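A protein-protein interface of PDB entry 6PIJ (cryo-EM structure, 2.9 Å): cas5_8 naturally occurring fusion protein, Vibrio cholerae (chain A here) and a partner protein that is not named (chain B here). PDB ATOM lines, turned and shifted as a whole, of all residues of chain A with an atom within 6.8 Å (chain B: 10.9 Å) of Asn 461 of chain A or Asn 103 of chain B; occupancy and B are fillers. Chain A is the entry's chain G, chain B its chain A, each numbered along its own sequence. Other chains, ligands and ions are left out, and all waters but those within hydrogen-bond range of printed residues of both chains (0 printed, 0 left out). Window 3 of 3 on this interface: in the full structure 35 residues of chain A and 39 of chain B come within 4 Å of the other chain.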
ATOM      1  N   THR A 179       0.812 -14.767 -37.564  1.00  0.00           N
ATOM      2  CA  THR A 179       0.569 -13.534 -36.770  1.00  0.00           C
ATOM      3  C   THR A 179       0.565 -13.931 -35.290  1.00  0.00           C
ATOM      4  O   THR A 179      -0.218 -14.830 -34.939  1.00  0.00           O
ATOM      5  CB  THR A 179      -0.737 -12.856 -37.200  1.00  0.00           C
ATOM      6  OG1 THR A 179      -0.615 -12.495 -38.577  1.00  0.00           O
ATOM      7  CG2 THR A 179      -1.070 -11.629 -36.379  1.00  0.00           C
ATOM      8  N   LEU A 180       1.402 -13.295 -34.465  1.00  0.00           N
ATOM      9  CA  LEU A 180       1.637 -13.695 -33.049  1.00  0.00           C
ATOM     10  C   LEU A 180       0.499 -13.214 -32.137  1.00  0.00           C
ATOM     11  O   LEU A 180       0.423 -13.729 -31.003  1.00  0.00           O
ATOM     12  CB  LEU A 180       2.989 -13.148 -32.577  1.00  0.00           C
ATOM     13  CG  LEU A 180       4.222 -13.714 -33.283  1.00  0.00           C
ATOM     14  CD1 LEU A 180       5.494 -13.118 -32.698  1.00  0.00           C
ATOM     15  CD2 LEU A 180       4.265 -15.232 -33.199  1.00  0.00           C
ATOM     16  N   ALA A 181      -0.345 -12.277 -32.589  1.00  0.00           N
ATOM     17  CA  ALA A 181      -1.515 -11.780 -31.824  1.00  0.00           C
ATOM     18  C   ALA A 181      -2.562 -11.176 -32.761  1.00  0.00           C
ATOM     19  O   ALA A 181      -2.213 -10.363 -33.615  1.00  0.00           O
ATOM     20  CB  ALA A 181      -1.060 -10.771 -30.799  1.00  0.00           C
ATOM     21  N   PRO A 182      -3.870 -11.519 -32.642  1.00  0.00           N
ATOM     22  CA  PRO A 182      -4.361 -12.552 -31.725  1.00  0.00           C
ATOM     23  C   PRO A 182      -4.181 -13.959 -32.316  1.00  0.00           C
ATOM     24  O   PRO A 182      -4.533 -14.157 -33.468  1.00  0.00           O
ATOM     25  CB  PRO A 182      -5.845 -12.195 -31.569  1.00  0.00           C
ATOM     26  CG  PRO A 182      -6.220 -11.601 -32.910  1.00  0.00           C
ATOM     27  CD  PRO A 182      -4.968 -10.899 -33.400  1.00  0.00           C
ATOM     28  N   GLN A 187       4.800 -19.420 -27.185  1.00  0.00           N
ATOM     29  CA  GLN A 187       6.077 -18.665 -27.348  1.00  0.00           C
ATOM     30  C   GLN A 187       6.756 -18.528 -25.982  1.00  0.00           C
ATOM     31  O   GLN A 187       6.082 -18.101 -25.022  1.00  0.00           O
ATOM     32  CB  GLN A 187       5.876 -17.297 -28.009  1.00  0.00           C
ATOM     33  CG  GLN A 187       4.641 -16.525 -27.562  1.00  0.00           C
ATOM     34  CD  GLN A 187       4.396 -15.312 -28.426  1.00  0.00           C
ATOM     35  OE1 GLN A 187       5.299 -14.792 -29.079  1.00  0.00           O
ATOM     36  NE2 GLN A 187       3.160 -14.837 -28.426  1.00  0.00           N
ATOM     37  N   ASP A 458      12.642  -9.360 -36.031  1.00  0.00           N
ATOM     38  CA  ASP A 458      11.889  -8.541 -35.043  1.00  0.00           C
ATOM     39  C   ASP A 458      10.402  -8.558 -35.425  1.00  0.00           C
ATOM     40  O   ASP A 458      10.034  -7.873 -36.401  1.00  0.00           O
ATOM     41  CB  ASP A 458      12.471  -7.126 -34.957  1.00  0.00           C
ATOM     42  CG  ASP A 458      12.100  -6.376 -33.688  1.00  0.00           C
ATOM     43  OD1 ASP A 458      10.895  -6.117 -33.490  1.00  0.00           O
ATOM     44  OD2 ASP A 458      13.018  -6.059 -32.906  1.00  0.00           O
ATOM     45  N   LYS A 459       9.591  -9.322 -34.681  1.00  0.00           N
ATOM     46  CA  LYS A 459       8.129  -9.499 -34.919  1.00  0.00           C
ATOM     47  C   LYS A 459       7.356  -8.433 -34.142  1.00  0.00           C
ATOM     48  O   LYS A 459       7.861  -7.911 -33.148  1.00  0.00           O
ATOM     49  CB  LYS A 459       7.681 -10.910 -34.520  1.00  0.00           C
ATOM     50  CG  LYS A 459       7.805 -11.966 -35.611  1.00  0.00           C
ATOM     51  CD  LYS A 459       6.696 -11.910 -36.639  1.00  0.00           C
ATOM     52  CE  LYS A 459       6.679 -13.119 -37.552  1.00  0.00           C
ATOM     53  NZ  LYS A 459       5.593 -13.030 -38.556  1.00  0.00           N
ATOM     54  N   PRO A 460       6.120  -8.066 -34.568  1.00  0.00           N
ATOM     55  CA  PRO A 460       5.303  -7.086 -33.846  1.00  0.00           C
ATOM     56  C   PRO A 460       4.997  -7.430 -32.377  1.00  0.00           C
ATOM     57  O   PRO A 460       5.148  -6.553 -31.544  1.00  0.00           O
ATOM     58  CB  PRO A 460       3.988  -7.047 -34.645  1.00  0.00           C
ATOM     59  CG  PRO A 460       4.387  -7.485 -36.033  1.00  0.00           C
ATOM     60  CD  PRO A 460       5.462  -8.526 -35.804  1.00  0.00           C
ATOM     61  N   ASN A 461       4.580  -8.674 -32.104  1.00  0.00           N
ATOM     62  CA  ASN A 461       4.131  -9.152 -30.766  1.00  0.00           C
ATOM     63  C   ASN A 461       4.968 -10.369 -30.344  1.00  0.00           C
ATOM     64  O   ASN A 461       4.376 -11.414 -29.999  1.00  0.00           O
ATOM     65  CB  ASN A 461       2.625  -9.440 -30.763  1.00  0.00           C
ATOM     66  CG  ASN A 461       1.782  -8.182 -30.785  1.00  0.00           C
ATOM     67  OD1 ASN A 461       1.791  -7.408 -29.831  1.00  0.00           O
ATOM     68  ND2 ASN A 461       1.043  -7.976 -31.863  1.00  0.00           N
ATOM     69  N   SER A 462       6.300 -10.236 -30.368  1.00  0.00           N
ATOM     70  CA  SER A 462       7.266 -11.213 -29.793  1.00  0.00           C
ATOM     71  C   SER A 462       7.219 -11.092 -28.265  1.00  0.00           C
ATOM     72  O   SER A 462       7.506  -9.988 -27.759  1.00  0.00           O
ATOM     73  CB  SER A 462       8.659 -10.992 -30.329  1.00  0.00           C
ATOM     74  OG  SER A 462       9.165  -9.724 -29.936  1.00  0.00           O
ATOM     75  N   LEU A 463       6.875 -12.177 -27.560  1.00  0.00           N
ATOM     76  CA  LEU A 463       6.365 -12.117 -26.161  1.00  0.00           C
ATOM     77  C   LEU A 463       7.514 -12.144 -25.145  1.00  0.00           C
ATOM     78  O   LEU A 463       7.709 -13.170 -24.468  1.00  0.00           O
ATOM     79  CB  LEU A 463       5.353 -13.243 -25.929  1.00  0.00           C
ATOM     80  CG  LEU A 463       4.401 -13.025 -24.752  1.00  0.00           C
ATOM     81  CD1 LEU A 463       3.002 -13.509 -25.098  1.00  0.00           C
ATOM     82  CD2 LEU A 463       4.908 -13.688 -23.475  1.00  0.00           C
ATOM     83  N   ARG A 464       8.297 -11.065 -25.151  1.00  0.00           N
ATOM     84  CA  ARG A 464       8.682 -10.248 -23.967  1.00  0.00           C
ATOM     85  C   ARG A 464       8.732  -8.801 -24.472  1.00  0.00           C
ATOM     86  O   ARG A 464       7.849  -8.004 -24.098  1.00  0.00           O
ATOM     87  CB  ARG A 464      10.011 -10.694 -23.343  1.00  0.00           C
ATOM     88  CG  ARG A 464      10.025 -12.092 -22.742  1.00  0.00           C
ATOM     89  CD  ARG A 464       8.989 -12.329 -21.658  1.00  0.00           C
ATOM     90  NE  ARG A 464       9.062 -13.683 -21.123  1.00  0.00           N
ATOM     91  CZ  ARG A 464       8.317 -14.157 -20.125  1.00  0.00           C
ATOM     92  NH1 ARG A 464       8.475 -15.409 -19.730  1.00  0.00           N
ATOM     93  NH2 ARG A 464       7.420 -13.391 -19.523  1.00  0.00           N
ATOM     94  N   HIS A 468      11.859 -12.857 -32.512  1.00  0.00           N
ATOM     95  CA  HIS A 468      11.084 -14.104 -32.755  1.00  0.00           C
ATOM     96  C   HIS A 468      11.612 -14.878 -33.967  1.00  0.00           C
ATOM     97  O   HIS A 468      11.712 -14.285 -35.060  1.00  0.00           O
ATOM     98  CB  HIS A 468       9.592 -13.791 -32.895  1.00  0.00           C
ATOM     99  CG  HIS A 468       8.729 -14.966 -32.588  1.00  0.00           C
ATOM    100  ND1 HIS A 468       8.111 -15.708 -33.573  1.00  0.00           N
ATOM    101  CD2 HIS A 468       8.414 -15.552 -31.413  1.00  0.00           C
ATOM    102  CE1 HIS A 468       7.436 -16.693 -33.016  1.00  0.00           C
ATOM    103  NE2 HIS A 468       7.602 -16.617 -31.691  1.00  0.00           N
ATOM    104  N   LYS B   1      -9.065  -0.309 -24.966  1.00  0.00           N
ATOM    105  CA  LYS B   1      -8.921  -1.178 -23.751  1.00  0.00           C
ATOM    106  C   LYS B   1      -8.812  -2.651 -24.163  1.00  0.00           C
ATOM    107  O   LYS B   1      -9.035  -2.946 -25.357  1.00  0.00           O
ATOM    108  CB  LYS B   1     -10.112  -0.995 -22.805  1.00  0.00           C
ATOM    109  CG  LYS B   1     -10.258   0.399 -22.212  1.00  0.00           C
ATOM    110  CD  LYS B   1     -11.403   0.523 -21.225  1.00  0.00           C
ATOM    111  CE  LYS B   1     -11.148  -0.161 -19.897  1.00  0.00           C
ATOM    112  NZ  LYS B   1     -10.049   0.477 -19.134  1.00  0.00           N
ATOM    113  N   LEU B   2      -8.501  -3.528 -23.199  1.00  0.00           N
ATOM    114  CA  LEU B   2      -8.332  -4.997 -23.382  1.00  0.00           C
ATOM    115  C   LEU B   2      -7.323  -5.238 -24.505  1.00  0.00           C
ATOM    116  O   LEU B   2      -7.714  -5.574 -25.621  1.00  0.00           O
ATOM    117  CB  LEU B   2      -9.694  -5.637 -23.688  1.00  0.00           C
ATOM    118  CG  LEU B   2     -10.520  -6.099 -22.486  1.00  0.00           C
ATOM    119  CD1 LEU B   2      -9.963  -7.390 -21.905  1.00  0.00           C
ATOM    120  CD2 LEU B   2     -10.609  -5.021 -21.415  1.00  0.00           C
ATOM    121  N   PRO B   3      -6.001  -5.054 -24.272  1.00  0.00           N
ATOM    122  CA  PRO B   3      -5.017  -5.180 -25.349  1.00  0.00           C
ATOM    123  C   PRO B   3      -4.932  -6.618 -25.884  1.00  0.00           C
ATOM    124  O   PRO B   3      -5.389  -7.529 -25.213  1.00  0.00           O
ATOM    125  CB  PRO B   3      -3.698  -4.736 -24.699  1.00  0.00           C
ATOM    126  CG  PRO B   3      -3.902  -5.022 -23.229  1.00  0.00           C
ATOM    127  CD  PRO B   3      -5.371  -4.746 -22.977  1.00  0.00           C
ATOM    128  N   THR B   4      -4.333  -6.782 -27.067  1.00  0.00           N
ATOM    129  CA  THR B   4      -4.280  -8.058 -27.835  1.00  0.00           C
ATOM    130  C   THR B   4      -3.441  -9.114 -27.096  1.00  0.00           C
ATOM    131  O   THR B   4      -3.464 -10.278 -27.543  1.00  0.00           O
ATOM    132  CB  THR B   4      -3.770  -7.818 -29.262  1.00  0.00           C
ATOM    133  OG1 THR B   4      -2.496  -7.176 -29.183  1.00  0.00           O
ATOM    134  CG2 THR B   4      -4.718  -6.975 -30.086  1.00  0.00           C
ATOM    135  N   ASN B   5      -2.723  -8.736 -26.027  1.00  0.00           N
ATOM    136  CA  ASN B   5      -2.009  -9.680 -25.124  1.00  0.00           C
ATOM    137  C   ASN B   5      -1.906  -9.088 -23.708  1.00  0.00           C
ATOM    138  O   ASN B   5      -0.968  -8.307 -23.460  1.00  0.00           O
ATOM    139  CB  ASN B   5      -0.652 -10.099 -25.705  1.00  0.00           C
ATOM    140  CG  ASN B   5       0.134  -8.972 -26.346  1.00  0.00           C
ATOM    141  OD1 ASN B   5      -0.437  -8.003 -26.840  1.00  0.00           O
ATOM    142  ND2 ASN B   5       1.450  -9.103 -26.361  1.00  0.00           N
ATOM    143  N   LEU B   6      -2.848  -9.453 -22.826  1.00  0.00           N
ATOM    144  CA  LEU B   6      -2.818  -9.199 -21.356  1.00  0.00           C
ATOM    145  C   LEU B   6      -3.029 -10.530 -20.625  1.00  0.00           C
ATOM    146  O   LEU B   6      -3.958 -11.272 -21.009  1.00  0.00           O
ATOM    147  CB  LEU B   6      -3.908  -8.182 -20.990  1.00  0.00           C
ATOM    148  CG  LEU B   6      -4.111  -7.904 -19.498  1.00  0.00           C
ATOM    149  CD1 LEU B   6      -2.854  -7.322 -18.870  1.00  0.00           C
ATOM    150  CD2 LEU B   6      -5.289  -6.968 -19.277  1.00  0.00           C
ATOM    151  N   ALA B   7      -2.210 -10.804 -19.603  1.00  0.00           N
ATOM    152  CA  ALA B   7      -2.197 -12.068 -18.828  1.00  0.00           C
ATOM    153  C   ALA B   7      -1.734 -11.812 -17.388  1.00  0.00           C
ATOM    154  O   ALA B   7      -1.216 -10.713 -17.104  1.00  0.00           O
ATOM    155  CB  ALA B   7      -1.315 -13.078 -19.518  1.00  0.00           C
ATOM    156  N   GLN B  98       1.203  -7.095 -10.655  1.00  0.00           N
ATOM    157  CA  GLN B  98       1.737  -6.779 -12.010  1.00  0.00           C
ATOM    158  C   GLN B  98       1.132  -7.722 -13.049  1.00  0.00           C
ATOM    159  O   GLN B  98       1.079  -8.929 -12.824  1.00  0.00           O
ATOM    160  CB  GLN B  98       3.263  -6.882 -12.007  1.00  0.00           C
ATOM    161  CG  GLN B  98       3.923  -6.137 -13.159  1.00  0.00           C
ATOM    162  CD  GLN B  98       5.431  -6.172 -13.098  1.00  0.00           C
ATOM    163  OE1 GLN B  98       6.029  -6.691 -12.157  1.00  0.00           O
ATOM    164  NE2 GLN B  98       6.066  -5.613 -14.116  1.00  0.00           N
ATOM    165  N   PRO B  99       0.650  -7.209 -14.208  1.00  0.00           N
ATOM    166  CA  PRO B  99       0.332  -8.061 -15.355  1.00  0.00           C
ATOM    167  C   PRO B  99       1.550  -8.861 -15.844  1.00  0.00           C
ATOM    168  O   PRO B  99       2.625  -8.289 -15.939  1.00  0.00           O
ATOM    169  CB  PRO B  99      -0.124  -7.075 -16.442  1.00  0.00           C
ATOM    170  CG  PRO B  99      -0.578  -5.853 -15.677  1.00  0.00           C
ATOM    171  CD  PRO B  99       0.330  -5.796 -14.466  1.00  0.00           C
ATOM    172  N   TYR B 100       1.349 -10.151 -16.132  1.00  0.00           N
ATOM    173  CA  TYR B 100       2.366 -11.086 -16.683  1.00  0.00           C
ATOM    174  C   TYR B 100       2.798 -10.630 -18.088  1.00  0.00           C
ATOM    175  O   TYR B 100       3.974 -10.852 -18.437  1.00  0.00           O
ATOM    176  CB  TYR B 100       1.818 -12.518 -16.680  1.00  0.00           C
ATOM    177  CG  TYR B 100       2.695 -13.550 -17.344  1.00  0.00           C
ATOM    178  CD1 TYR B 100       3.774 -14.115 -16.682  1.00  0.00           C
ATOM    179  CD2 TYR B 100       2.440 -13.972 -18.640  1.00  0.00           C
ATOM    180  CE1 TYR B 100       4.578 -15.068 -17.289  1.00  0.00           C
ATOM    181  CE2 TYR B 100       3.236 -14.920 -19.263  1.00  0.00           C
ATOM    182  CZ  TYR B 100       4.309 -15.473 -18.586  1.00  0.00           C
ATOM    183  OH  TYR B 100       5.095 -16.408 -19.195  1.00  0.00           O
ATOM    184  N   LYS B 101       1.888 -10.006 -18.851  1.00  0.00           N
ATOM    185  CA  LYS B 101       2.091  -9.589 -20.269  1.00  0.00           C
ATOM    186  C   LYS B 101       2.066  -8.054 -20.387  1.00  0.00           C
ATOM    187  O   LYS B 101       1.941  -7.379 -19.344  1.00  0.00           O
ATOM    188  CB  LYS B 101       1.039 -10.271 -21.152  1.00  0.00           C
ATOM    189  CG  LYS B 101       1.441 -11.628 -21.714  1.00  0.00           C
ATOM    190  CD  LYS B 101       0.580 -12.063 -22.881  1.00  0.00           C
ATOM    191  CE  LYS B 101       0.188 -13.525 -22.851  1.00  0.00           C
ATOM    192  NZ  LYS B 101      -0.430 -13.947 -24.130  1.00  0.00           N
ATOM    193  N   CYS B 102       2.176  -7.539 -21.620  1.00  0.00           N
ATOM    194  CA  CYS B 102       2.555  -6.142 -21.969  1.00  0.00           C
ATOM    195  C   CYS B 102       1.508  -5.515 -22.907  1.00  0.00           C
ATOM    196  O   CYS B 102       0.317  -5.854 -22.761  1.00  0.00           O
ATOM    197  CB  CYS B 102       3.934  -6.164 -22.621  1.00  0.00           C
ATOM    198  SG  CYS B 102       4.719  -4.535 -22.736  1.00  0.00           S
ATOM    199  N   ASN B 103       1.934  -4.582 -23.774  1.00  0.00           N
ATOM    200  CA  ASN B 103       1.221  -4.094 -24.992  1.00  0.00           C
ATOM    201  C   ASN B 103       0.236  -2.959 -24.661  1.00  0.00           C
ATOM    202  O   ASN B 103      -0.442  -2.492 -25.600  1.00  0.00           O
ATOM    203  CB  ASN B 103       0.520  -5.235 -25.743  1.00  0.00           C
ATOM    204  CG  ASN B 103       0.113  -4.880 -27.161  1.00  0.00           C
ATOM    205  OD1 ASN B 103       0.790  -4.111 -27.840  1.00  0.00           O
ATOM    206  ND2 ASN B 103      -0.995  -5.440 -27.618  1.00  0.00           N
ATOM    207  N   SER B 104       0.157  -2.505 -23.404  1.00  0.00           N
ATOM    208  CA  SER B 104      -0.688  -1.353 -22.993  1.00  0.00           C
ATOM    209  C   SER B 104      -0.188  -0.764 -21.669  1.00  0.00           C
ATOM    210  O   SER B 104      -0.638  -1.229 -20.599  1.00  0.00           O
ATOM    211  CB  SER B 104      -2.143  -1.744 -22.918  1.00  0.00           C
ATOM    212  OG  SER B 104      -2.957  -0.610 -22.662  1.00  0.00           O
ATOM    213  N   SER B 105       0.703   0.231 -21.755  1.00  0.00           N
ATOM    214  CA  SER B 105       1.228   1.027 -20.613  1.00  0.00           C
ATOM    215  C   SER B 105       0.062   1.648 -19.830  1.00  0.00           C
ATOM    216  O   SER B 105       0.133   1.646 -18.582  1.00  0.00           O
ATOM    217  CB  SER B 105       2.197   2.083 -21.084  1.00  0.00           C
ATOM    218  OG  SER B 105       3.255   1.503 -21.834  1.00  0.00           O
ATOM    219  N   LYS B 106      -0.967   2.132 -20.539  1.00  0.00           N
ATOM    220  CA  LYS B 106      -2.205   2.734 -19.968  1.00  0.00           C
ATOM    221  C   LYS B 106      -2.916   1.706 -19.077  1.00  0.00           C
ATOM    222  O   LYS B 106      -3.075   1.978 -17.868  1.00  0.00           O
ATOM    223  CB  LYS B 106      -3.130   3.225 -21.091  1.00  0.00           C
ATOM    224  CG  LYS B 106      -4.424   3.899 -20.648  1.00  0.00           C
ATOM    225  CD  LYS B 106      -4.224   5.107 -19.750  1.00  0.00           C
ATOM    226  CE  LYS B 106      -5.523   5.732 -19.286  1.00  0.00           C
ATOM    227  NZ  LYS B 106      -6.251   6.394 -20.395  1.00  0.00           N
ATOM    228  N   VAL B 107      -3.315   0.566 -19.653  1.00  0.00           N
ATOM    229  CA  VAL B 107      -4.064  -0.523 -18.951  1.00  0.00           C
ATOM    230  C   VAL B 107      -3.179  -1.084 -17.826  1.00  0.00           C
ATOM    231  O   VAL B 107      -3.719  -1.323 -16.721  1.00  0.00           O
ATOM    232  CB  VAL B 107      -4.540  -1.610 -19.940  1.00  0.00           C
ATOM    233  CG1 VAL B 107      -5.102  -2.841 -19.244  1.00  0.00           C
ATOM    234  CG2 VAL B 107      -5.571  -1.061 -20.917  1.00  0.00           C
ATOM    235  N   LYS B 108      -1.873  -1.248 -18.083  1.00  0.00           N
ATOM    236  CA  LYS B 108      -0.872  -1.741 -17.094  1.00  0.00           C
ATOM    237  C   LYS B 108      -0.859  -0.822 -15.866  1.00  0.00           C
ATOM    238  O   LYS B 108      -0.995  -1.351 -14.740  1.00  0.00           O
ATOM    239  CB  LYS B 108       0.525  -1.831 -17.719  1.00  0.00           C
ATOM    240  CG  LYS B 108       1.582  -2.500 -16.849  1.00  0.00           C
ATOM    241  CD  LYS B 108       2.851  -2.848 -17.600  1.00  0.00           C
ATOM    242  CE  LYS B 108       3.807  -3.698 -16.789  1.00  0.00           C
ATOM    243  NZ  LYS B 108       4.448  -2.922 -15.701  1.00  0.00           N
ATOM    244  N   GLN B 109      -0.713   0.495 -16.069  1.00  0.00           N
ATOM    245  CA  GLN B 109      -0.666   1.495 -14.965  1.00  0.00           C
ATOM    246  C   GLN B 109      -2.061   1.633 -14.331  1.00  0.00           C
ATOM    247  O   GLN B 109      -2.115   1.902 -13.114  1.00  0.00           O
ATOM    248  CB  GLN B 109      -0.086   2.839 -15.427  1.00  0.00           C
ATOM    249  CG  GLN B 109      -0.998   3.672 -16.320  1.00  0.00           C
ATOM    250  CD  GLN B 109      -0.436   5.039 -16.632  1.00  0.00           C
ATOM    251  OE1 GLN B 109       0.602   5.448 -16.115  1.00  0.00           O
ATOM    252  NE2 GLN B 109      -1.128   5.765 -17.495  1.00  0.00           N
ATOM    253  N   PHE B 346      -6.837 -12.430 -20.179  1.00  0.00           N
ATOM    254  CA  PHE B 346      -7.804 -11.299 -20.202  1.00  0.00           C
ATOM    255  C   PHE B 346      -7.632 -10.539 -21.521  1.00  0.00           C
ATOM    256  O   PHE B 346      -7.292  -9.337 -21.513  1.00  0.00           O
ATOM    257  CB  PHE B 346      -7.625 -10.395 -18.976  1.00  0.00           C
ATOM    258  CG  PHE B 346      -7.491 -11.102 -17.648  1.00  0.00           C
ATOM    259  CD1 PHE B 346      -8.209 -12.257 -17.366  1.00  0.00           C
ATOM    260  CD2 PHE B 346      -6.661 -10.587 -16.662  1.00  0.00           C
ATOM    261  CE1 PHE B 346      -8.085 -12.886 -16.135  1.00  0.00           C
ATOM    262  CE2 PHE B 346      -6.538 -11.219 -15.433  1.00  0.00           C
ATOM    263  CZ  PHE B 346      -7.251 -12.367 -15.171  1.00  0.00           C
ATOM    264  N   GLN B 347      -7.894 -11.239 -22.627  1.00  0.00           N
ATOM    265  CA  GLN B 347      -7.329 -10.942 -23.970  1.00  0.00           C
ATOM    266  C   GLN B 347      -8.420 -10.851 -25.049  1.00  0.00           C
ATOM    267  O   GLN B 347      -8.196 -10.092 -26.015  1.00  0.00           O
ATOM    268  CB  GLN B 347      -6.315 -12.043 -24.290  1.00  0.00           C
ATOM    269  CG  GLN B 347      -5.200 -11.616 -25.233  1.00  0.00           C
ATOM    270  CD  GLN B 347      -4.052 -12.598 -25.248  1.00  0.00           C
ATOM    271  OE1 GLN B 347      -3.579 -13.054 -24.208  1.00  0.00           O
ATOM    272  NE2 GLN B 347      -3.575 -12.916 -26.440  1.00  0.00           N
ATOM    273  N   HIS B 348      -9.564 -11.531 -24.866  1.00  0.00           N
ATOM    274  CA  HIS B 348     -10.419 -12.138 -25.929  1.00  0.00           C
ATOM    275  C   HIS B 348      -9.900 -11.754 -27.327  1.00  0.00           C
ATOM    276  O   HIS B 348      -8.899 -12.372 -27.744  1.00  0.00           O
ATOM    277  CB  HIS B 348     -11.922 -11.910 -25.649  1.00  0.00           C
ATOM    278  CG  HIS B 348     -12.406 -10.498 -25.710  1.00  0.00           C
ATOM    279  ND1 HIS B 348     -13.453 -10.119 -26.532  1.00  0.00           N
ATOM    280  CD2 HIS B 348     -12.001  -9.376 -25.075  1.00  0.00           C
ATOM    281  CE1 HIS B 348     -13.671  -8.827 -26.400  1.00  0.00           C
ATOM    282  NE2 HIS B 348     -12.794  -8.348 -25.510  1.00  0.00           N
ATOM    283  N   LYS B 349     -10.530 -10.794 -28.021  1.00  0.00           N
ATOM    284  CA  LYS B 349     -10.154 -10.289 -29.373  1.00  0.00           C
ATOM    285  C   LYS B 349      -9.643 -11.435 -30.261  1.00  0.00           C
ATOM    286  O   LYS B 349      -8.695 -11.201 -31.031  1.00  0.00           O
ATOM    287  CB  LYS B 349      -9.118  -9.168 -29.224  1.00  0.00           C
ATOM    288  CG  LYS B 349      -9.636  -7.899 -28.561  1.00  0.00           C
ATOM    289  CD  LYS B 349      -8.633  -6.765 -28.563  1.00  0.00           C
ATOM    290  CE  LYS B 349      -9.257  -5.429 -28.221  1.00  0.00           C
ATOM    291  NZ  LYS B 349      -8.232  -4.369 -28.074  1.00  0.00           N
ATOM    292  N   ASP B 351      -8.250 -14.468 -28.992  1.00  0.00           N
ATOM    293  CA  ASP B 351      -7.595 -15.320 -27.960  1.00  0.00           C
ATOM    294  C   ASP B 351      -8.427 -15.279 -26.673  1.00  0.00           C
ATOM    295  O   ASP B 351      -8.891 -16.310 -26.185  1.00  0.00           O
ATOM    296  CB  ASP B 351      -6.144 -14.891 -27.712  1.00  0.00           C
ATOM    297  CG  ASP B 351      -5.304 -15.896 -26.936  1.00  0.00           C
ATOM    298  OD1 ASP B 351      -5.796 -17.015 -26.676  1.00  0.00           O
ATOM    299  OD2 ASP B 351      -4.154 -15.554 -26.598  1.00  0.00           O
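O of Leu 2 of chain B is in hydrogen-bond range of NZ of Lys 349 of chain B (2.8 Å).
The side-chain amide oxygen (OD1) of Asn 5 of chain B sits close to the side-chain hydroxyl (OG1) of Thr 4 of chain B (3.2 Å).
OG1 of Thr 4 of chain B lies within hydrogen-bond range of ND2 of Asn 103 of chain B (2.8 Å).
OD1 of Asn 5 of chain B sits at hydrogen-bond distance from ND2 of Asn 103 of chain B.
O of Ala 7 of chain B sits at hydrogen-bond distance from N of Tyr 100 of chain B (2.8 Å).
The side-chain amino group (NZ) of Lys 101 of chain B is in hydrogen-bond range of the side-chain amide oxygen (OE1) of Gln 347 of chain B.
Among the printed residues, pairs that only touch across the chains: Pro 182 of chain A with Lys 349 of chain B, Arg 464 of chain A with Tyr 100 of chain B, Leu 463 of chain A with Lys 101 of chain B, Asn 461 of chain A with Asn 5 of chain B and Asn 461 of chain A with Asn 103 of chain B.
Of chain B, only Asn 5 and Asn 103 come within 4 Å of Asn 461 of chain A.
Leu 180 of chain A touches none of the printed residues of chain B.
No residue of chain B comes within 4 Å of Ala 181 of chain A.
No residue of chain B comes within 4 Å of Pro 460 of chain A.
Ser 462 of chain A touches none of the printed residues of chain B.
Of the printed residues of chain A, Tyr 100 of chain B touches Arg 464 (3.6 Å).
Of the printed residues of chain B, Leu 463 of chain A touches Lys 101.
Printed residues of chain A within 4 Å of Lys 101 of chain B: Leu 463.
Printed residues of chain A within 4 Å of Lys 349 of chain B: Pro 182.
Printed residues of chain A that touch a printed residue of chain B: Pro 182, Asn 461, Leu 463 and Arg 464.
Hydrophobic or aromatic side chains of chain A that line the printed part of chain B: Pro 182 and Leu 463.
Of the 24 printed residues of chain B, 5 touch a printed residue of chain A.
Among the printed residues, 5 pairs touch across the chains.
Among the printed residues, no Asp or Glu carboxylate lies within 4 Å of a Lys or Arg side-chain nitrogen of the other chain.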
